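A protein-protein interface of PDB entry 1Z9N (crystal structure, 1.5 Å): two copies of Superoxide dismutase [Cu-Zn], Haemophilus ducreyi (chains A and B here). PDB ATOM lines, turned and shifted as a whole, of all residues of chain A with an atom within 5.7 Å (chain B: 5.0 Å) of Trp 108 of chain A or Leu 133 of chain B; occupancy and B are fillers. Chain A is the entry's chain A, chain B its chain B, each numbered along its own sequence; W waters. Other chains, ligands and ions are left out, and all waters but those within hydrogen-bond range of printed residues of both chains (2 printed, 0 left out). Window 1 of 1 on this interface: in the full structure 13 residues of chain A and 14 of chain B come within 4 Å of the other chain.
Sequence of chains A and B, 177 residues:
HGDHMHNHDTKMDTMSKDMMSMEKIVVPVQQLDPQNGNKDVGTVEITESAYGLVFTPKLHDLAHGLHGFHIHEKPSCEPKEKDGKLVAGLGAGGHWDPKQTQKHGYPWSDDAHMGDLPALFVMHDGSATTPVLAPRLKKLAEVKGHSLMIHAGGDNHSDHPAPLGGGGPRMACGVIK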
ATOM      1  N   TYR A 106     -19.118 -25.426  11.740  1.00  0.00           N
ATOM      2  CA  TYR A 106     -18.796 -24.096  12.268  1.00  0.00           C
ATOM      3  C   TYR A 106     -17.365 -23.717  11.912  1.00  0.00           C
ATOM      4  O   TYR A 106     -16.506 -24.587  11.749  1.00  0.00           O
ATOM      5  CB  TYR A 106     -19.042 -24.062  13.768  1.00  0.00           C
ATOM      6  CG  TYR A 106     -20.506 -23.870  14.110  1.00  0.00           C
ATOM      7  CD1 TYR A 106     -21.246 -24.912  14.661  1.00  0.00           C
ATOM      8  CD2 TYR A 106     -21.161 -22.662  13.853  1.00  0.00           C
ATOM      9  CE1 TYR A 106     -22.590 -24.762  14.971  1.00  0.00           C
ATOM     10  CE2 TYR A 106     -22.524 -22.498  14.154  1.00  0.00           C
ATOM     11  CZ  TYR A 106     -23.223 -23.552  14.724  1.00  0.00           C
ATOM     12  OH  TYR A 106     -24.557 -23.431  15.039  1.00  0.00           O
ATOM     13  N   PRO A 107     -17.068 -22.421  11.811  1.00  0.00           N
ATOM     14  CA  PRO A 107     -15.715 -21.987  11.494  1.00  0.00           C
ATOM     15  C   PRO A 107     -14.661 -22.352  12.525  1.00  0.00           C
ATOM     16  O   PRO A 107     -13.458 -22.392  12.225  1.00  0.00           O
ATOM     17  CB  PRO A 107     -15.837 -20.470  11.393  1.00  0.00           C
ATOM     18  CG  PRO A 107     -17.271 -20.234  11.098  1.00  0.00           C
ATOM     19  CD  PRO A 107     -18.037 -21.305  11.819  1.00  0.00           C
ATOM     20  N   TRP A 108     -15.105 -22.585  13.754  1.00  0.00           N
ATOM     21  CA  TRP A 108     -14.241 -22.983  14.890  1.00  0.00           C
ATOM     22  C   TRP A 108     -14.228 -24.482  15.181  1.00  0.00           C
ATOM     23  O   TRP A 108     -13.741 -24.897  16.263  1.00  0.00           O
ATOM     24  CB  TRP A 108     -14.695 -22.250  16.152  1.00  0.00           C
ATOM     25  CG  TRP A 108     -16.162 -22.283  16.341  1.00  0.00           C
ATOM     26  CD1 TRP A 108     -16.894 -23.273  16.952  1.00  0.00           C
ATOM     27  CD2 TRP A 108     -17.100 -21.265  15.961  1.00  0.00           C
ATOM     28  NE1 TRP A 108     -18.226 -22.948  16.956  1.00  0.00           N
ATOM     29  CE2 TRP A 108     -18.374 -21.722  16.346  1.00  0.00           C
ATOM     30  CE3 TRP A 108     -16.992 -20.035  15.322  1.00  0.00           C
ATOM     31  CZ2 TRP A 108     -19.525 -20.967  16.142  1.00  0.00           C
ATOM     32  CZ3 TRP A 108     -18.151 -19.294  15.111  1.00  0.00           C
ATOM     33  CH2 TRP A 108     -19.366 -19.755  15.548  1.00  0.00           C
ATOM     34  N   SER A 109     -14.826 -25.274  14.306  1.00  0.00           N
ATOM     35  CA  SER A 109     -14.838 -26.735  14.450  1.00  0.00           C
ATOM     36  C   SER A 109     -13.848 -27.410  13.514  1.00  0.00           C
ATOM     37  O   SER A 109     -13.842 -27.182  12.317  1.00  0.00           O
ATOM     38  CB  SER A 109     -16.213 -27.289  14.171  1.00  0.00           C
ATOM     39  OG  SER A 109     -16.112 -28.701  14.225  1.00  0.00           O
ATOM     40  N   ASP A 110     -13.021 -28.295  14.085  1.00  0.00           N
ATOM     41  CA  ASP A 110     -12.070 -29.046  13.273  1.00  0.00           C
ATOM     42  C   ASP A 110     -12.712 -30.144  12.468  1.00  0.00           C
ATOM     43  O   ASP A 110     -12.054 -30.729  11.614  1.00  0.00           O
ATOM     44  CB  ASP A 110     -10.942 -29.578  14.161  1.00  0.00           C
ATOM     45  CG  ASP A 110     -10.015 -28.485  14.602  1.00  0.00           C
ATOM     46  OD1 ASP A 110      -9.730 -27.573  13.804  1.00  0.00           O
ATOM     47  OD2 ASP A 110      -9.507 -28.477  15.746  1.00  0.00           O
ATOM     48  N   PRO A 118     -17.842 -17.646   8.829  1.00  0.00           N
ATOM     49  CA  PRO A 118     -19.080 -17.109   9.367  1.00  0.00           C
ATOM     50  C   PRO A 118     -19.909 -16.510   8.245  1.00  0.00           C
ATOM     51  O   PRO A 118     -19.361 -16.054   7.236  1.00  0.00           O
ATOM     52  CB  PRO A 118     -18.610 -16.038  10.380  1.00  0.00           C
ATOM     53  CG  PRO A 118     -17.177 -16.366  10.704  1.00  0.00           C
ATOM     54  CD  PRO A 118     -16.645 -16.987   9.396  1.00  0.00           C
ATOM     55  N   LEU A 133     -14.160 -13.470  11.026  1.00  0.00           N
ATOM     56  CA  LEU A 133     -12.896 -14.189  11.276  1.00  0.00           C
ATOM     57  C   LEU A 133     -13.042 -15.673  10.942  1.00  0.00           C
ATOM     58  O   LEU A 133     -14.004 -16.332  11.323  1.00  0.00           O
ATOM     59  CB  LEU A 133     -12.591 -14.068  12.752  1.00  0.00           C
ATOM     60  CG  LEU A 133     -11.290 -14.723  13.250  1.00  0.00           C
ATOM     61  CD1 LEU A 133     -10.071 -13.985  12.752  1.00  0.00           C
ATOM     62  CD2 LEU A 133     -11.267 -14.908  14.749  1.00  0.00           C
ATOM     63  N   PRO A 135     -10.896 -18.579  12.188  1.00  0.00           N
ATOM     64  CA  PRO A 135      -9.768 -18.779  13.095  1.00  0.00           C
ATOM     65  C   PRO A 135      -8.851 -19.907  12.670  1.00  0.00           C
ATOM     66  O   PRO A 135      -7.698 -19.921  13.130  1.00  0.00           O
ATOM     67  CB  PRO A 135     -10.438 -19.150  14.414  1.00  0.00           C
ATOM     68  CG  PRO A 135     -11.766 -19.659  14.055  1.00  0.00           C
ATOM     69  CD  PRO A 135     -12.199 -18.908  12.830  1.00  0.00           C
ATOM     70  N   ARG A 136      -9.332 -20.847  11.890  1.00  0.00           N
ATOM     71  CA  ARG A 136      -8.509 -21.996  11.525  1.00  0.00           C
ATOM     72  C   ARG A 136      -7.515 -21.684  10.436  1.00  0.00           C
ATOM     73  O   ARG A 136      -6.566 -22.468  10.217  1.00  0.00           O
ATOM     74  CB  ARG A 136      -9.394 -23.151  11.084  1.00  0.00           C
ATOM     75  CG  ARG A 136     -10.151 -23.739  12.211  1.00  0.00           C
ATOM     76  CD  ARG A 136     -10.896 -25.001  11.846  1.00  0.00           C
ATOM     77  NE  ARG A 136     -12.060 -24.645  11.085  1.00  0.00           N
ATOM     78  CZ  ARG A 136     -12.604 -25.343  10.078  1.00  0.00           C
ATOM     79  NH1 ARG A 136     -12.067 -26.486   9.641  1.00  0.00           N
ATOM     80  NH2 ARG A 136     -13.709 -24.870   9.519  1.00  0.00           N
ATOM     81  N   SER B  49     -14.331 -23.680  22.516  1.00  0.00           N
ATOM     82  CA  SER B  49     -13.903 -24.329  21.284  1.00  0.00           C
ATOM     83  C   SER B  49     -12.392 -24.335  21.286  1.00  0.00           C
ATOM     84  O   SER B  49     -11.719 -23.727  22.131  1.00  0.00           O
ATOM     85  CB  SER B  49     -14.410 -23.604  20.036  1.00  0.00           C
ATOM     86  OG  SER B  49     -13.578 -22.497  19.716  1.00  0.00           O
ATOM     87  N   ALA B  50     -11.830 -25.013  20.307  1.00  0.00           N
ATOM     88  CA  ALA B  50     -10.393 -25.016  20.157  1.00  0.00           C
ATOM     89  C   ALA B  50      -9.816 -23.661  19.776  1.00  0.00           C
ATOM     90  O   ALA B  50      -8.596 -23.479  19.787  1.00  0.00           O
ATOM     91  CB  ALA B  50      -9.969 -26.054  19.129  1.00  0.00           C
ATOM     92  N   TYR B  51     -10.695 -22.716  19.379  1.00  0.00           N
ATOM     93  CA  TYR B  51     -10.264 -21.407  18.890  1.00  0.00           C
ATOM     94  C   TYR B  51     -10.850 -20.246  19.693  1.00  0.00           C
ATOM     95  O   TYR B  51     -10.782 -19.117  19.243  1.00  0.00           O
ATOM     96  CB  TYR B  51     -10.603 -21.235  17.407  1.00  0.00           C
ATOM     97  CG  TYR B  51      -9.998 -22.355  16.600  1.00  0.00           C
ATOM     98  CD1 TYR B  51     -10.679 -23.524  16.414  1.00  0.00           C
ATOM     99  CD2 TYR B  51      -8.690 -22.263  16.140  1.00  0.00           C
ATOM    100  CE1 TYR B  51     -10.100 -24.590  15.734  1.00  0.00           C
ATOM    101  CE2 TYR B  51      -8.103 -23.304  15.460  1.00  0.00           C
ATOM    102  CZ  TYR B  51      -8.812 -24.462  15.278  1.00  0.00           C
ATOM    103  OH  TYR B  51      -8.279 -25.545  14.581  1.00  0.00           O
ATOM    104  N   GLY B  52     -11.407 -20.543  20.858  1.00  0.00           N
ATOM    105  CA  GLY B  52     -11.908 -19.525  21.779  1.00  0.00           C
ATOM    106  C   GLY B  52     -13.326 -19.794  22.212  1.00  0.00           C
ATOM    107  O   GLY B  52     -13.965 -20.783  21.793  1.00  0.00           O
ATOM    108  N   LEU B  53     -13.856 -18.897  23.026  1.00  0.00           N
ATOM    109  CA  LEU B  53     -15.207 -19.066  23.521  1.00  0.00           C
ATOM    110  C   LEU B  53     -16.258 -18.788  22.473  1.00  0.00           C
ATOM    111  O   LEU B  53     -16.166 -17.804  21.724  1.00  0.00           O
ATOM    112  CB  LEU B  53     -15.503 -18.190  24.741  1.00  0.00           C
ATOM    113  CG  LEU B  53     -14.611 -18.462  25.969  1.00  0.00           C
ATOM    114  CD1 LEU B  53     -15.119 -17.604  27.131  1.00  0.00           C
ATOM    115  CD2 LEU B  53     -14.597 -19.897  26.357  1.00  0.00           C
ATOM    116  N   VAL B  54     -17.272 -19.638  22.443  1.00  0.00           N
ATOM    117  CA  VAL B  54     -18.406 -19.518  21.508  1.00  0.00           C
ATOM    118  C   VAL B  54     -19.628 -19.100  22.313  1.00  0.00           C
ATOM    119  O   VAL B  54     -19.957 -19.702  23.343  1.00  0.00           O
ATOM    120  CB  VAL B  54     -18.653 -20.857  20.771  1.00  0.00           C
ATOM    121  CG1 VAL B  54     -19.828 -20.779  19.809  1.00  0.00           C
ATOM    122  CG2 VAL B  54     -17.386 -21.271  20.019  1.00  0.00           C
ATOM    123  N   PRO B 107     -12.986  -8.135  17.762  1.00  0.00           N
ATOM    124  CA  PRO B 107     -12.744  -9.241  18.677  1.00  0.00           C
ATOM    125  C   PRO B 107     -11.368  -9.880  18.503  1.00  0.00           C
ATOM    126  O   PRO B 107     -10.875 -10.513  19.405  1.00  0.00           O
ATOM    127  CB  PRO B 107     -13.876 -10.222  18.348  1.00  0.00           C
ATOM    128  CG  PRO B 107     -14.941  -9.338  17.880  1.00  0.00           C
ATOM    129  CD  PRO B 107     -14.237  -8.324  16.998  1.00  0.00           C
ATOM    130  N   PRO B 118     -18.192 -10.295  18.460  1.00  0.00           N
ATOM    131  CA  PRO B 118     -18.946 -10.047  17.220  1.00  0.00           C
ATOM    132  C   PRO B 118     -20.398  -9.707  17.537  1.00  0.00           C
ATOM    133  O   PRO B 118     -20.908 -10.108  18.565  1.00  0.00           O
ATOM    134  CB  PRO B 118     -18.779 -11.347  16.437  1.00  0.00           C
ATOM    135  CG  PRO B 118     -17.601 -12.034  17.029  1.00  0.00           C
ATOM    136  CD  PRO B 118     -17.671 -11.681  18.490  1.00  0.00           C
ATOM    137  N   PRO B 131     -24.459 -18.146  16.347  1.00  0.00           N
ATOM    138  CA  PRO B 131     -23.336 -18.115  17.281  1.00  0.00           C
ATOM    139  C   PRO B 131     -22.181 -17.269  16.766  1.00  0.00           C
ATOM    140  O   PRO B 131     -21.984 -17.126  15.549  1.00  0.00           O
ATOM    141  CB  PRO B 131     -22.904 -19.592  17.406  1.00  0.00           C
ATOM    142  CG  PRO B 131     -23.867 -20.303  16.771  1.00  0.00           C
ATOM    143  CD  PRO B 131     -24.615 -19.471  15.728  1.00  0.00           C
ATOM    144  N   VAL B 132     -21.408 -16.764  17.711  1.00  0.00           N
ATOM    145  CA  VAL B 132     -20.199 -15.991  17.402  1.00  0.00           C
ATOM    146  C   VAL B 132     -19.040 -16.420  18.270  1.00  0.00           C
ATOM    147  O   VAL B 132     -19.255 -16.937  19.359  1.00  0.00           O
ATOM    148  CB  VAL B 132     -20.434 -14.461  17.568  1.00  0.00           C
ATOM    149  CG1 VAL B 132     -21.572 -13.993  16.661  1.00  0.00           C
ATOM    150  CG2 VAL B 132     -20.776 -14.120  19.040  1.00  0.00           C
ATOM    151  N   LEU B 133     -17.827 -16.194  17.758  1.00  0.00           N
ATOM    152  CA  LEU B 133     -16.588 -16.581  18.424  1.00  0.00           C
ATOM    153  C   LEU B 133     -15.878 -15.364  19.037  1.00  0.00           C
ATOM    154  O   LEU B 133     -15.719 -14.363  18.371  1.00  0.00           O
ATOM    155  CB  LEU B 133     -15.681 -17.172  17.379  1.00  0.00           C
ATOM    156  CG  LEU B 133     -14.341 -17.690  17.905  1.00  0.00           C
ATOM    157  CD1 LEU B 133     -14.570 -18.909  18.838  1.00  0.00           C
ATOM    158  CD2 LEU B 133     -13.403 -18.008  16.739  1.00  0.00           C
ATOM    159  N   ALA B 134     -15.340 -15.516  20.249  1.00  0.00           N
ATOM    160  CA  ALA B 134     -14.395 -14.573  20.864  1.00  0.00           C
ATOM    161  C   ALA B 134     -13.016 -15.244  20.913  1.00  0.00           C
ATOM    162  O   ALA B 134     -12.728 -15.980  21.874  1.00  0.00           O
ATOM    163  CB  ALA B 134     -14.829 -14.197  22.247  1.00  0.00           C
ATOM    164  N   PRO B 135     -12.178 -15.001  19.909  1.00  0.00           N
ATOM    165  CA  PRO B 135     -10.963 -15.788  19.761  1.00  0.00           C
ATOM    166  C   PRO B 135      -9.950 -15.546  20.873  1.00  0.00           C
ATOM    167  O   PRO B 135      -9.021 -16.389  21.011  1.00  0.00           O
ATOM    168  CB  PRO B 135     -10.388 -15.319  18.428  1.00  0.00           C
ATOM    169  CG  PRO B 135     -10.920 -13.964  18.256  1.00  0.00           C
ATOM    170  CD  PRO B 135     -12.333 -14.043  18.788  1.00  0.00           C
HETATM  171  O   HOH W   1      -7.319 -27.531  16.851  1.00  0.00           O
HETATM  172  O   HOH W   2     -13.337 -26.520  18.428  1.00  0.00           O
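The side-chain hydroxyl (OH) of Tyr 51 of chain B lies within hydrogen-bond range of the side-chain carboxylate (OD1) of Asp 110 of chain A (2.6 Å).
NE of Arg 136 of chain A sits at hydrogen-bond distance from O of Pro 107 of chain A (2.9 Å). OG of Ser 49 of chain B is in hydrogen-bond range of N of Tyr 51 of chain B, at 2.9 Å. O of Ser 109 of chain A lies close to NH1 of Arg 136 of chain A (3.3 Å). The side-chain hydroxyl of Ser 49 of chain B lies within hydrogen-bond range of the backbone carbonyl oxygen of Gly 52 of chain B (2.7 Å).
Among the printed residues, pairs that only touch across the chains: Tyr 106 of chain A with Pro 131 of chain B, Trp 108 of chain A with Ser 49 of chain B, Trp 108 of chain A with Tyr 51 of chain B, Trp 108 of chain A with Val 54 of chain B, Trp 108 of chain A with Pro 131 of chain B, Trp 108 of chain A with Leu 133 of chain B, Leu 133 of chain A with Pro 135 of chain B, Pro 135 of chain A with Tyr 51 of chain B, Pro 135 of chain A with Leu 133 of chain B and Arg 136 of chain A with Tyr 51 of chain B.
Of chain B, only Ser 49, Tyr 51, Val 54, Pro 131 and Leu 133 come within 4 Å of Trp 108 of chain A. Of chain A, only Trp 108 and Pro 135 come within 4 Å of Leu 133 of chain B. Printed residues of chain A within 4 Å of Pro 135 of chain B: Leu 133 (3.6 Å). Printed residues of chain B within 4 Å of Leu 133 of chain A: Pro 135. Of the printed residues of chain A, Pro 131 of chain B touches Tyr 106 and Trp 108. The nearest residue of chain B that does not touch Trp 108 of chain A is Val 132 of chain B (4.2 Å). The nearest residue of chain A that does not touch Leu 133 of chain B is Leu 133 of chain A (4.3 Å). The nearest printed residue of chain B that does not touch Leu 133 of chain A is Leu 133 of chain B (4.3 Å).
Hydrophobic or aromatic side chains of chain B within 4 Å of the printed part of chain A: Tyr 51, Val 54, Pro 131, Leu 133 and Pro 135. Of the 9 printed residues of chain A, 6 touch a printed residue of chain B. Hydrophobic or aromatic side chains of chain A within 4 Å of the printed part of chain B: Tyr 106, Trp 108, Leu 133 and Pro 135. Along chain A the printed residues that touch a printed residue of chain B span positions 106 to 136. Among the printed residues, no Asp or Glu carboxylate lies within 4 Å of a Lys or Arg side-chain nitrogen of the other chain.
Leu 133 of chain A touches Pro 135 of chain B, and with the chains exchanged Pro 135 of chain A touches Leu 133 of chain B.
Water W1 lies within hydrogen-bond range of OD2 of Asp 110 of chain A (2.6 Å) and OH of Tyr 51 of chain B (3.2 Å). Water W2 bridges O of Trp 108 of chain A (2.7 Å) and N of Ala 50 of chain B (2.8 Å).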
